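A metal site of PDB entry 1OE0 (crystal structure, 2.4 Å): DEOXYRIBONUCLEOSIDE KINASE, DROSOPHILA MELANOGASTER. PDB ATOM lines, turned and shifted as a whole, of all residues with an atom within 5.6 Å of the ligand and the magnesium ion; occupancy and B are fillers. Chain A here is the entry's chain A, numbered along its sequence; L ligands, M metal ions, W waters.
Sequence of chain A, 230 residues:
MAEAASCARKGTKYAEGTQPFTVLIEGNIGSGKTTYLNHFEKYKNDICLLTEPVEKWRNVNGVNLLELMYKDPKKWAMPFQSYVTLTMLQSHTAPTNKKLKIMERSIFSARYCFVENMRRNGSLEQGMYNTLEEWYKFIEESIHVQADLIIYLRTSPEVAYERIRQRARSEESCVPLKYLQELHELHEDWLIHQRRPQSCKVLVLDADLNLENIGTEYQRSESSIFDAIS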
ATOM      1  N   GLY A  27       6.372  21.843   8.998  1.00  0.00           N
ATOM      2  CA  GLY A  27       6.442  21.603   7.569  1.00  0.00           C
ATOM      3  C   GLY A  27       7.854  21.143   7.240  1.00  0.00           C
ATOM      4  O   GLY A  27       8.785  21.373   8.016  1.00  0.00           O
ATOM      5  N   ASN A  28       8.021  20.513   6.093  1.00  0.00           N
ATOM      6  CA  ASN A  28       9.327  20.015   5.687  1.00  0.00           C
ATOM      7  C   ASN A  28      10.335  21.137   5.543  1.00  0.00           C
ATOM      8  O   ASN A  28       9.960  22.316   5.551  1.00  0.00           O
ATOM      9  CB  ASN A  28       9.205  19.291   4.346  1.00  0.00           C
ATOM     10  CG  ASN A  28      10.306  18.274   4.129  1.00  0.00           C
ATOM     11  OD1 ASN A  28      11.367  18.333   4.748  1.00  0.00           O
ATOM     12  ND2 ASN A  28      10.058  17.334   3.219  1.00  0.00           N
ATOM     13  N   ILE A  29      11.607  20.788   5.410  1.00  0.00           N
ATOM     14  CA  ILE A  29      12.640  21.794   5.219  1.00  0.00           C
ATOM     15  C   ILE A  29      12.269  22.558   3.953  1.00  0.00           C
ATOM     16  O   ILE A  29      11.936  21.960   2.928  1.00  0.00           O
ATOM     17  CB  ILE A  29      14.021  21.151   4.992  1.00  0.00           C
ATOM     18  CG1 ILE A  29      14.367  20.218   6.153  1.00  0.00           C
ATOM     19  CG2 ILE A  29      15.081  22.235   4.847  1.00  0.00           C
ATOM     20  CD1 ILE A  29      15.655  19.443   5.935  1.00  0.00           C
ATOM     21  N   GLY A  30      12.343  23.880   4.014  1.00  0.00           N
ATOM     22  CA  GLY A  30      12.035  24.681   2.843  1.00  0.00           C
ATOM     23  C   GLY A  30      10.571  24.745   2.476  1.00  0.00           C
ATOM     24  O   GLY A  30      10.246  25.152   1.372  1.00  0.00           O
ATOM     25  N   SER A  31       9.677  24.325   3.365  1.00  0.00           N
ATOM     26  CA  SER A  31       8.251  24.372   3.080  1.00  0.00           C
ATOM     27  C   SER A  31       7.703  25.800   3.200  1.00  0.00           C
ATOM     28  O   SER A  31       6.577  26.083   2.788  1.00  0.00           O
ATOM     29  CB  SER A  31       7.492  23.447   4.026  1.00  0.00           C
ATOM     30  OG  SER A  31       7.690  23.819   5.382  1.00  0.00           O
ATOM     31  N   GLY A  32       8.513  26.704   3.758  1.00  0.00           N
ATOM     32  CA  GLY A  32       8.075  28.088   3.911  1.00  0.00           C
ATOM     33  C   GLY A  32       7.535  28.454   5.280  1.00  0.00           C
ATOM     34  O   GLY A  32       6.671  29.336   5.390  1.00  0.00           O
ATOM     35  N   LYS A  33       8.026  27.815   6.334  1.00  0.00           N
ATOM     36  CA  LYS A  33       7.562  28.109   7.686  1.00  0.00           C
ATOM     37  C   LYS A  33       7.896  29.532   8.096  1.00  0.00           C
ATOM     38  O   LYS A  33       7.069  30.217   8.704  1.00  0.00           O
ATOM     39  CB  LYS A  33       8.166  27.119   8.701  1.00  0.00           C
ATOM     40  CG  LYS A  33       7.734  25.672   8.498  1.00  0.00           C
ATOM     41  CD  LYS A  33       8.378  24.730   9.513  1.00  0.00           C
ATOM     42  CE  LYS A  33       9.891  24.627   9.339  1.00  0.00           C
ATOM     43  NZ  LYS A  33      10.281  24.024   8.023  1.00  0.00           N
ATOM     44  N   THR A  34       9.108  29.984   7.784  1.00  0.00           N
ATOM     45  CA  THR A  34       9.520  31.344   8.140  1.00  0.00           C
ATOM     46  C   THR A  34       8.763  32.372   7.317  1.00  0.00           C
ATOM     47  O   THR A  34       8.279  33.373   7.846  1.00  0.00           O
ATOM     48  CB  THR A  34      11.036  31.519   7.919  1.00  0.00           C
ATOM     49  OG1 THR A  34      11.745  30.583   8.733  1.00  0.00           O
ATOM     50  CG2 THR A  34      11.471  32.946   8.294  1.00  0.00           C
ATOM     51  N   THR A  35       8.639  32.109   6.009  1.00  0.00           N
ATOM     52  CA  THR A  35       7.913  33.007   5.105  1.00  0.00           C
ATOM     53  C   THR A  35       6.500  33.225   5.620  1.00  0.00           C
ATOM     54  O   THR A  35       5.999  34.345   5.636  1.00  0.00           O
ATOM     55  CB  THR A  35       7.813  32.405   3.687  1.00  0.00           C
ATOM     56  OG1 THR A  35       9.122  32.284   3.114  1.00  0.00           O
ATOM     57  CG2 THR A  35       6.942  33.275   2.801  1.00  0.00           C
ATOM     58  N   GLU A  52      12.799  31.228  12.874  1.00  0.00           N
ATOM     59  CA  GLU A  52      14.123  30.855  12.383  1.00  0.00           C
ATOM     60  C   GLU A  52      15.113  30.388  13.451  1.00  0.00           C
ATOM     61  O   GLU A  52      16.177  30.983  13.623  1.00  0.00           O
ATOM     62  CB  GLU A  52      14.713  32.039  11.613  1.00  0.00           C
ATOM     63  CG  GLU A  52      15.776  31.661  10.576  1.00  0.00           C
ATOM     64  CD  GLU A  52      15.197  30.915   9.371  1.00  0.00           C
ATOM     65  OE1 GLU A  52      15.503  31.313   8.225  1.00  0.00           O
ATOM     66  OE2 GLU A  52      14.453  29.919   9.584  1.00  0.00           O
ATOM     67  N   VAL A  54      17.091  28.018  13.376  1.00  0.00           N
ATOM     68  CA  VAL A  54      18.321  27.553  12.728  1.00  0.00           C
ATOM     69  C   VAL A  54      19.503  28.462  12.988  1.00  0.00           C
ATOM     70  O   VAL A  54      20.644  27.993  13.051  1.00  0.00           O
ATOM     71  CB  VAL A  54      18.152  27.466  11.206  1.00  0.00           C
ATOM     72  CG1 VAL A  54      19.099  26.430  10.644  1.00  0.00           C
ATOM     73  CG2 VAL A  54      16.698  27.166  10.871  1.00  0.00           C
ATOM     74  N   TRP A  57      21.507  27.321  15.835  1.00  0.00           N
ATOM     75  CA  TRP A  57      22.247  26.083  15.575  1.00  0.00           C
ATOM     76  C   TRP A  57      23.473  26.310  14.683  1.00  0.00           C
ATOM     77  O   TRP A  57      24.431  25.554  14.729  1.00  0.00           O
ATOM     78  CB  TRP A  57      21.323  25.033  14.932  1.00  0.00           C
ATOM     79  CG  TRP A  57      19.999  24.929  15.617  1.00  0.00           C
ATOM     80  CD1 TRP A  57      19.731  25.223  16.928  1.00  0.00           C
ATOM     81  CD2 TRP A  57      18.758  24.537  15.027  1.00  0.00           C
ATOM     82  NE1 TRP A  57      18.395  25.047  17.183  1.00  0.00           N
ATOM     83  CE2 TRP A  57      17.774  24.627  16.046  1.00  0.00           C
ATOM     84  CE3 TRP A  57      18.381  24.113  13.760  1.00  0.00           C
ATOM     85  CZ2 TRP A  57      16.431  24.318  15.819  1.00  0.00           C
ATOM     86  CZ3 TRP A  57      17.043  23.813  13.533  1.00  0.00           C
ATOM     87  CH2 TRP A  57      16.086  23.912  14.561  1.00  0.00           C
ATOM     88  N   LEU A  66      25.110  22.937  12.877  1.00  0.00           N
ATOM     89  CA  LEU A  66      24.366  22.500  11.696  1.00  0.00           C
ATOM     90  C   LEU A  66      25.328  21.982  10.646  1.00  0.00           C
ATOM     91  O   LEU A  66      25.121  20.927  10.052  1.00  0.00           O
ATOM     92  CB  LEU A  66      23.557  23.650  11.110  1.00  0.00           C
ATOM     93  CG  LEU A  66      22.729  23.245   9.899  1.00  0.00           C
ATOM     94  CD1 LEU A  66      21.733  22.191  10.317  1.00  0.00           C
ATOM     95  CD2 LEU A  66      22.019  24.468   9.330  1.00  0.00           C
ATOM     96  N   MET A  69      27.079  18.690  11.695  1.00  0.00           N
ATOM     97  CA  MET A  69      26.171  17.557  11.606  1.00  0.00           C
ATOM     98  C   MET A  69      26.090  17.023  10.184  1.00  0.00           C
ATOM     99  O   MET A  69      26.148  15.820   9.976  1.00  0.00           O
ATOM    100  CB  MET A  69      24.773  17.956  12.096  1.00  0.00           C
ATOM    101  CG  MET A  69      23.728  16.837  12.009  1.00  0.00           C
ATOM    102  SD  MET A  69      22.912  16.740  10.381  1.00  0.00           S
ATOM    103  CE  MET A  69      21.788  18.159  10.485  1.00  0.00           C
ATOM    104  N   TYR A  70      25.960  17.917   9.199  1.00  0.00           N
ATOM    105  CA  TYR A  70      25.874  17.476   7.813  1.00  0.00           C
ATOM    106  C   TYR A  70      27.175  16.878   7.286  1.00  0.00           C
ATOM    107  O   TYR A  70      27.151  15.959   6.463  1.00  0.00           O
ATOM    108  CB  TYR A  70      25.435  18.644   6.921  1.00  0.00           C
ATOM    109  CG  TYR A  70      23.938  18.845   6.898  1.00  0.00           C
ATOM    110  CD1 TYR A  70      23.375  20.084   7.221  1.00  0.00           C
ATOM    111  CD2 TYR A  70      23.080  17.793   6.580  1.00  0.00           C
ATOM    112  CE1 TYR A  70      21.993  20.262   7.208  1.00  0.00           C
ATOM    113  CE2 TYR A  70      21.698  17.970   6.567  1.00  0.00           C
ATOM    114  CZ  TYR A  70      21.166  19.204   6.878  1.00  0.00           C
ATOM    115  OH  TYR A  70      19.801  19.383   6.852  1.00  0.00           O
ATOM    116  N   PHE A  80      24.129  17.672  18.020  1.00  0.00           N
ATOM    117  CA  PHE A  80      23.302  18.615  17.297  1.00  0.00           C
ATOM    118  C   PHE A  80      21.820  18.517  17.699  1.00  0.00           C
ATOM    119  O   PHE A  80      21.209  19.522  18.041  1.00  0.00           O
ATOM    120  CB  PHE A  80      23.404  18.390  15.784  1.00  0.00           C
ATOM    121  CG  PHE A  80      22.458  19.256  14.979  1.00  0.00           C
ATOM    122  CD1 PHE A  80      22.648  20.628  14.883  1.00  0.00           C
ATOM    123  CD2 PHE A  80      21.357  18.691  14.354  1.00  0.00           C
ATOM    124  CE1 PHE A  80      21.766  21.419  14.172  1.00  0.00           C
ATOM    125  CE2 PHE A  80      20.452  19.482  13.635  1.00  0.00           C
ATOM    126  CZ  PHE A  80      20.664  20.854  13.547  1.00  0.00           C
ATOM    127  N   GLN A  81      21.262  17.296  17.657  1.00  0.00           N
ATOM    128  CA  GLN A  81      19.856  17.102  18.022  1.00  0.00           C
ATOM    129  C   GLN A  81      19.619  17.428  19.489  1.00  0.00           C
ATOM    130  O   GLN A  81      18.567  17.918  19.858  1.00  0.00           O
ATOM    131  CB  GLN A  81      19.401  15.664  17.697  1.00  0.00           C
ATOM    132  CG  GLN A  81      19.259  15.417  16.202  1.00  0.00           C
ATOM    133  CD  GLN A  81      18.258  16.349  15.551  1.00  0.00           C
ATOM    134  OE1 GLN A  81      18.402  16.706  14.381  1.00  0.00           O
ATOM    135  NE2 GLN A  81      17.223  16.751  16.304  1.00  0.00           N
ATOM    136  N   VAL A  84      19.268  21.110  19.456  1.00  0.00           N
ATOM    137  CA  VAL A  84      17.999  21.506  18.841  1.00  0.00           C
ATOM    138  C   VAL A  84      16.897  21.343  19.909  1.00  0.00           C
ATOM    139  O   VAL A  84      16.069  22.220  20.107  1.00  0.00           O
ATOM    140  CB  VAL A  84      17.626  20.599  17.634  1.00  0.00           C
ATOM    141  CG1 VAL A  84      16.159  20.789  17.287  1.00  0.00           C
ATOM    142  CG2 VAL A  84      18.489  20.937  16.428  1.00  0.00           C
ATOM    143  N   GLU A 104       8.135  28.634  15.103  1.00  0.00           N
ATOM    144  CA  GLU A 104       8.591  27.877  13.930  1.00  0.00           C
ATOM    145  C   GLU A 104       9.219  26.593  14.461  1.00  0.00           C
ATOM    146  O   GLU A 104      10.196  26.642  15.216  1.00  0.00           O
ATOM    147  CB  GLU A 104       9.606  28.675  13.097  1.00  0.00           C
ATOM    148  CG  GLU A 104       9.967  28.041  11.766  1.00  0.00           C
ATOM    149  CD  GLU A 104      10.978  28.841  10.976  1.00  0.00           C
ATOM    150  OE1 GLU A 104      11.007  30.077  11.132  1.00  0.00           O
ATOM    151  OE2 GLU A 104      11.747  28.238  10.194  1.00  0.00           O
ATOM    152  N   ARG A 105       8.667  25.450  14.066  1.00  0.00           N
ATOM    153  CA  ARG A 105       9.179  24.180  14.558  1.00  0.00           C
ATOM    154  C   ARG A 105       8.809  23.990  16.020  1.00  0.00           C
ATOM    155  O   ARG A 105       8.215  24.859  16.649  1.00  0.00           O
ATOM    156  CB  ARG A 105      10.698  24.098  14.426  1.00  0.00           C
ATOM    157  CG  ARG A 105      11.185  23.780  13.035  1.00  0.00           C
ATOM    158  CD  ARG A 105      10.660  22.441  12.577  1.00  0.00           C
ATOM    159  NE  ARG A 105      11.213  22.070  11.287  1.00  0.00           N
ATOM    160  CZ  ARG A 105      10.674  21.135  10.503  1.00  0.00           C
ATOM    161  NH1 ARG A 105       9.583  20.501  10.907  1.00  0.00           N
ATOM    162  NH2 ARG A 105      11.225  20.846   9.321  1.00  0.00           N
ATOM    163  N   SER A 106       9.188  22.834  16.573  1.00  0.00           N
ATOM    164  CA  SER A 106       8.892  22.503  17.943  1.00  0.00           C
ATOM    165  C   SER A 106       9.720  21.305  18.356  1.00  0.00           C
ATOM    166  O   SER A 106      10.394  20.682  17.547  1.00  0.00           O
ATOM    167  CB  SER A 106       7.411  22.162  18.092  1.00  0.00           C
ATOM    168  OG  SER A 106       7.110  20.973  17.378  1.00  0.00           O
ATOM    169  N   SER A 109       8.679  17.955  16.305  1.00  0.00           N
ATOM    170  CA  SER A 109       9.145  17.638  14.969  1.00  0.00           C
ATOM    171  C   SER A 109      10.596  17.203  15.047  1.00  0.00           C
ATOM    172  O   SER A 109      11.060  16.429  14.224  1.00  0.00           O
ATOM    173  CB  SER A 109       8.977  18.846  14.031  1.00  0.00           C
ATOM    174  OG  SER A 109       9.481  20.030  14.618  1.00  0.00           O
ATOM    175  N   ALA A 110      11.300  17.711  16.049  1.00  0.00           N
ATOM    176  CA  ALA A 110      12.703  17.325  16.219  1.00  0.00           C
ATOM    177  C   ALA A 110      12.744  15.854  16.589  1.00  0.00           C
ATOM    178  O   ALA A 110      13.577  15.091  16.078  1.00  0.00           O
ATOM    179  CB  ALA A 110      13.353  18.156  17.325  1.00  0.00           C
ATOM    180  N   ARG A 111      11.822  15.437  17.461  1.00  0.00           N
ATOM    181  CA  ARG A 111      11.756  14.056  17.916  1.00  0.00           C
ATOM    182  C   ARG A 111      11.156  13.090  16.894  1.00  0.00           C
ATOM    183  O   ARG A 111      11.807  12.130  16.475  1.00  0.00           O
ATOM    184  CB  ARG A 111      10.934  13.958  19.201  1.00  0.00           C
ATOM    185  CG  ARG A 111      10.802  12.546  19.745  1.00  0.00           C
ATOM    186  CD  ARG A 111       9.884  12.461  20.951  1.00  0.00           C
ATOM    187  NE  ARG A 111      10.057  11.178  21.638  1.00  0.00           N
ATOM    188  CZ  ARG A 111       9.404  10.809  22.742  1.00  0.00           C
ATOM    189  NH1 ARG A 111       8.516  11.613  23.295  1.00  0.00           N
ATOM    190  NH2 ARG A 111       9.656   9.639  23.307  1.00  0.00           N
ATOM    191  N   PHE A 114      12.981  14.342  12.648  1.00  0.00           N
ATOM    192  CA  PHE A 114      14.416  14.324  12.484  1.00  0.00           C
ATOM    193  C   PHE A 114      15.182  13.268  13.252  1.00  0.00           C
ATOM    194  O   PHE A 114      16.014  12.581  12.665  1.00  0.00           O
ATOM    195  CB  PHE A 114      14.986  15.713  12.772  1.00  0.00           C
ATOM    196  CG  PHE A 114      14.537  16.749  11.788  1.00  0.00           C
ATOM    197  CD1 PHE A 114      13.342  17.419  11.977  1.00  0.00           C
ATOM    198  CD2 PHE A 114      15.267  16.975  10.629  1.00  0.00           C
ATOM    199  CE1 PHE A 114      12.868  18.299  11.009  1.00  0.00           C
ATOM    200  CE2 PHE A 114      14.800  17.851   9.653  1.00  0.00           C
ATOM    201  CZ  PHE A 114      13.607  18.510   9.851  1.00  0.00           C
ATOM    202  N   VAL A 115      14.930  13.137  14.556  1.00  0.00           N
ATOM    203  CA  VAL A 115      15.637  12.122  15.317  1.00  0.00           C
ATOM    204  C   VAL A 115      15.282  10.740  14.783  1.00  0.00           C
ATOM    205  O   VAL A 115      16.153   9.887  14.601  1.00  0.00           O
ATOM    206  CB  VAL A 115      15.295  12.189  16.836  1.00  0.00           C
ATOM    207  CG1 VAL A 115      15.840  10.953  17.549  1.00  0.00           C
ATOM    208  CG2 VAL A 115      15.898  13.447  17.440  1.00  0.00           C
ATOM    209  N   MET A 118      17.032  10.033  11.518  1.00  0.00           N
ATOM    210  CA  MET A 118      18.463   9.825  11.743  1.00  0.00           C
ATOM    211  C   MET A 118      18.733   8.469  12.372  1.00  0.00           C
ATOM    212  O   MET A 118      19.834   7.926  12.244  1.00  0.00           O
ATOM    213  CB  MET A 118      19.027  10.941  12.624  1.00  0.00           C
ATOM    214  CG  MET A 118      19.096  12.269  11.903  1.00  0.00           C
ATOM    215  SD  MET A 118      19.700  13.593  12.944  1.00  0.00           S
ATOM    216  CE  MET A 118      19.519  15.016  11.821  1.00  0.00           C
ATOM    217  N   LEU A 153       2.363  23.175   6.991  1.00  0.00           N
ATOM    218  CA  LEU A 153       2.558  23.670   5.638  1.00  0.00           C
ATOM    219  C   LEU A 153       2.951  22.482   4.772  1.00  0.00           C
ATOM    220  O   LEU A 153       4.132  22.178   4.593  1.00  0.00           O
ATOM    221  CB  LEU A 153       3.671  24.741   5.605  1.00  0.00           C
ATOM    222  CG  LEU A 153       3.491  25.967   6.506  1.00  0.00           C
ATOM    223  CD1 LEU A 153       4.617  26.946   6.224  1.00  0.00           C
ATOM    224  CD2 LEU A 153       2.153  26.632   6.244  1.00  0.00           C
ATOM    225  N   ARG A 167      17.577  29.220  -1.562  1.00  0.00           N
ATOM    226  CA  ARG A 167      18.022  29.877  -0.341  1.00  0.00           C
ATOM    227  C   ARG A 167      19.551  29.751  -0.263  1.00  0.00           C
ATOM    228  O   ARG A 167      20.245  30.665   0.179  1.00  0.00           O
ATOM    229  CB  ARG A 167      17.369  29.220   0.881  1.00  0.00           C
ATOM    230  CG  ARG A 167      17.772  29.778   2.241  1.00  0.00           C
ATOM    231  CD  ARG A 167      16.816  29.227   3.311  1.00  0.00           C
ATOM    232  NE  ARG A 167      16.835  27.770   3.365  1.00  0.00           N
ATOM    233  CZ  ARG A 167      15.828  27.026   3.797  1.00  0.00           C
ATOM    234  NH1 ARG A 167      14.698  27.591   4.212  1.00  0.00           N
ATOM    235  NH2 ARG A 167      15.947  25.698   3.836  1.00  0.00           N
ATOM    236  N   ARG A 169      21.754  27.787   1.630  1.00  0.00           N
ATOM    237  CA  ARG A 169      22.518  27.777   2.884  1.00  0.00           C
ATOM    238  C   ARG A 169      23.673  26.832   2.588  1.00  0.00           C
ATOM    239  O   ARG A 169      23.473  25.710   2.134  1.00  0.00           O
ATOM    240  CB  ARG A 169      21.698  27.215   4.044  1.00  0.00           C
ATOM    241  CG  ARG A 169      20.597  28.116   4.581  1.00  0.00           C
ATOM    242  CD  ARG A 169      19.884  27.420   5.744  1.00  0.00           C
ATOM    243  NE  ARG A 169      18.771  28.204   6.288  1.00  0.00           N
ATOM    244  CZ  ARG A 169      17.633  27.662   6.732  1.00  0.00           C
ATOM    245  NH1 ARG A 169      17.468  26.342   6.713  1.00  0.00           N
ATOM    246  NH2 ARG A 169      16.667  28.447   7.181  1.00  0.00           N
ATOM    247  N   GLU A 172      23.422  23.241   3.798  1.00  0.00           N
ATOM    248  CA  GLU A 172      22.441  22.399   3.116  1.00  0.00           C
ATOM    249  C   GLU A 172      22.771  22.070   1.656  1.00  0.00           C
ATOM    250  O   GLU A 172      21.973  21.415   0.968  1.00  0.00           O
ATOM    251  CB  GLU A 172      21.064  23.081   3.198  1.00  0.00           C
ATOM    252  CG  GLU A 172      20.378  22.904   4.549  1.00  0.00           C
ATOM    253  CD  GLU A 172      19.339  23.970   4.853  1.00  0.00           C
ATOM    254  OE1 GLU A 172      18.644  24.435   3.916  1.00  0.00           O
ATOM    255  OE2 GLU A 172      19.215  24.344   6.035  1.00  0.00           O
ATOM    256  N   VAL A 175      22.227  18.292   0.702  1.00  0.00           N
ATOM    257  CA  VAL A 175      20.982  17.611   1.047  1.00  0.00           C
ATOM    258  C   VAL A 175      20.289  17.013  -0.176  1.00  0.00           C
ATOM    259  O   VAL A 175      19.810  17.729  -1.056  1.00  0.00           O
ATOM    260  CB  VAL A 175      19.994  18.582   1.759  1.00  0.00           C
ATOM    261  CG1 VAL A 175      18.732  17.833   2.158  1.00  0.00           C
ATOM    262  CG2 VAL A 175      20.652  19.187   2.972  1.00  0.00           C
ATOM    263  N   TYR A 179      16.322  12.488   1.089  1.00  0.00           N
ATOM    264  CA  TYR A 179      16.280  12.927   2.464  1.00  0.00           C
ATOM    265  C   TYR A 179      14.994  13.678   2.699  1.00  0.00           C
ATOM    266  O   TYR A 179      14.282  13.416   3.676  1.00  0.00           O
ATOM    267  CB  TYR A 179      17.483  13.825   2.770  1.00  0.00           C
ATOM    268  CG  TYR A 179      17.667  14.162   4.226  1.00  0.00           C
ATOM    269  CD1 TYR A 179      17.845  13.152   5.187  1.00  0.00           C
ATOM    270  CD2 TYR A 179      17.710  15.487   4.662  1.00  0.00           C
ATOM    271  CE1 TYR A 179      18.059  13.458   6.520  1.00  0.00           C
ATOM    272  CE2 TYR A 179      17.915  15.810   6.007  1.00  0.00           C
ATOM    273  CZ  TYR A 179      18.091  14.789   6.926  1.00  0.00           C
ATOM    274  OH  TYR A 179      18.320  15.076   8.255  1.00  0.00           O
HETATM  275  P1  LIG L   1      13.799  23.677   9.344  1.00  0.00           P
HETATM  276  O1  LIG L   1      13.626  23.500  10.806  1.00  0.00           O
HETATM  277  O2  LIG L   1      12.826  23.039   8.443  1.00  0.00           O
HETATM  278  O3  LIG L   1      13.842  25.230   9.019  1.00  0.00           O
HETATM  279  P2  LIG L   1      13.945  25.973   7.613  1.00  0.00           P
HETATM  280  O4  LIG L   1      14.249  27.364   7.930  1.00  0.00           O
HETATM  281  O5  LIG L   1      14.941  25.252   6.764  1.00  0.00           O
HETATM  282  O6  LIG L   1      12.457  25.887   7.055  1.00  0.00           O
HETATM  283  P3  LIG L   1      11.431  26.860   6.179  1.00  0.00           P
HETATM  284  O7  LIG L   1      12.063  27.111   4.869  1.00  0.00           O
HETATM  285  O8  LIG L   1      10.092  26.206   6.139  1.00  0.00           O
HETATM  286  O9  LIG L   1      11.344  28.206   7.016  1.00  0.00           O
HETATM  287  O10 LIG L   1      15.217  23.132   8.865  1.00  0.00           O
HETATM  288  C1  LIG L   1      16.418  23.909   9.206  1.00  0.00           C
HETATM  289  C2  LIG L   1      17.692  23.021   9.101  1.00  0.00           C
HETATM  290  O11 LIG L   1      17.823  22.322  10.323  1.00  0.00           O
HETATM  291  C3  LIG L   1      17.609  21.946   8.020  1.00  0.00           C
HETATM  292  O12 LIG L   1      18.877  21.822   7.374  1.00  0.00           O
HETATM  293  C4  LIG L   1      17.167  20.675   8.780  1.00  0.00           C
HETATM  294  C5  LIG L   1      17.784  20.934  10.147  1.00  0.00           C
HETATM  295  N1  LIG L   1      16.990  20.404  11.349  1.00  0.00           N
HETATM  296  C6  LIG L   1      17.577  19.197  11.886  1.00  0.00           C
HETATM  297  O13 LIG L   1      18.617  18.677  11.412  1.00  0.00           O
HETATM  298  N2  LIG L   1      16.968  18.649  12.998  1.00  0.00           N
HETATM  299  C7  LIG L   1      15.859  19.173  13.538  1.00  0.00           C
HETATM  300  O14 LIG L   1      15.372  18.528  14.615  1.00  0.00           O
HETATM  301  C8  LIG L   1      15.243  20.383  12.998  1.00  0.00           C
HETATM  302  C9  LIG L   1      13.991  20.970  13.601  1.00  0.00           C
HETATM  303  C10 LIG L   1      15.852  20.921  11.909  1.00  0.00           C
HETATM  304 MG    MG M   1      12.810  28.864   8.438  1.00  0.00          MG
HETATM  305  O   HOH W   1      18.703  17.678   8.733  1.00  0.00           O
HETATM  306  O   HOH W   2      10.926  27.898   2.419  1.00  0.00           O
HETATM  307  O   HOH W   3      13.535  29.865   6.702  1.00  0.00           O
HETATM  308  O   HOH W   4      10.110  29.899   4.698  1.00  0.00           O
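N2 of the ligand is in hydrogen-bond range of OE1 of Gln 81, 2.8 Å away. An oxygen (O8) of the ligand lies within hydrogen-bond range of the backbone NH of Gly 32 (2.9 Å). OG of Ser 31 sits at hydrogen-bond distance from O8 of the ligand (3.5 Å). OH of Tyr 70 sits at hydrogen-bond distance from O12 of the ligand (2.7 Å). NE of Arg 105 is in salt-bridge range of O1 of the ligand, at 2.8 Å. An oxygen (O9) of the ligand sits close to the backbone NH (N) of Thr 34. The side-chain carboxylate (OE2) of Glu 172 sits at hydrogen-bond distance from an oxygen (O12) of the ligand (2.9 Å). An oxygen (O2) of the ligand is in salt-bridge range of the side-chain amino group (NZ) of Lys 33, 2.8 Å away. N of Lys 33 is in hydrogen-bond range of O8 of the ligand (2.6 Å). N of Gly 30 lies close to O7 of the ligand, 3.4 Å away. The backbone NH (N) of Ser 31 lies within hydrogen-bond range of an oxygen (O8) of the ligand. O5 of the ligand is in salt-bridge range of NH1 of Arg 169, at 2.8 Å. NH1 of Arg 167 lies within salt-bridge range of O7 of the ligand, at 2.8 Å.
OE1 of Glu 172 lies within salt-bridge range of NH2 of Arg 167 (3.0 Å). The side-chain amide oxygen of Gln 81 lies close to the side-chain sulfur of Met 118 (3.7 Å). The backbone carbonyl oxygen (O) of Ser 109 lies within hydrogen-bond range of the backbone NH (N) of Phe 114, at 3.2 Å. The side-chain carboxylate (OE2) of Glu 172 is in salt-bridge range of the guanidinium group (NH1) of Arg 169 (2.7 Å). O of Trp 57 sits at hydrogen-bond distance from N of Leu 66 (3.3 Å). NH2 of Arg 169 lies within salt-bridge range of OE1 of Glu 52. The backbone carbonyl oxygen of Asn 28 sits at hydrogen-bond distance from the side-chain amino group of Lys 33 (3.0 Å). The backbone NH (N) of Val 115 lies within hydrogen-bond range of the backbone carbonyl oxygen (O) of Ala 110 (2.8 Å).
Asn 28 touches the ligand (O to O8, 3.9 Å). CD1 of Ile 29 touches C4 of the ligand (3.4 Å). CG2 of Val 54 touches C1 of the ligand, 3.7 Å away. Trp 57 touches the ligand. CD1 of Leu 66 touches O11 of the ligand (3.9 Å). Met 69 touches the ligand. Phe 80 touches the ligand. CG1 of Val 84 touches O14 of the ligand (3.6 Å). CA of Ala 110 touches O14 of the ligand (3.3 Å). Phe 114 touches the ligand. Met 118 touches the ligand. Hydrophobic or aromatic side chains that line the ligand: Ile 29, Val 54, Trp 57, Leu 66, Met 69, Tyr 70, Phe 80, Val 84, Ala 110, Phe 114 and Met 118. 24 residues have an atom within 4 Å of the ligand: Asn 28, Ile 29, Gly 30, Ser 31, Gly 32, Lys 33, Thr 34, Glu 52, Val 54, Trp 57, Leu 66, Met 69, Tyr 70, Phe 80, Gln 81, Val 84, Glu 104, Arg 105, Ala 110, Phe 114, Met 118, Arg 167, Arg 169 and Glu 172.
Within 4 Å of the magnesium ion: Thr 34, Glu 52 and Glu 104.
The magnesium ion is bound by OG1 of Thr 34, water W3, O4 of the ligand, OE2 of Glu 104, O9 of the ligand and OE2 of Glu 52. The magnesium ion has six donor atoms within binding distance.
Water W3 lies within hydrogen-bond range of OE1 of Glu 52 and NH2 of Arg 169. Water W2 lies within hydrogen-bond range of an oxygen (O7) of the ligand (2.8 Å), the backbone NH (N) of Gly 32 (3.0 Å) and the backbone carbonyl oxygen (O) of Gly 30 (3.0 Å). Water W1 lies within hydrogen-bond range of OH of Tyr 179 (2.7 Å), OH of Tyr 70 (2.8 Å) and O13 of the ligand (2.9 Å).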
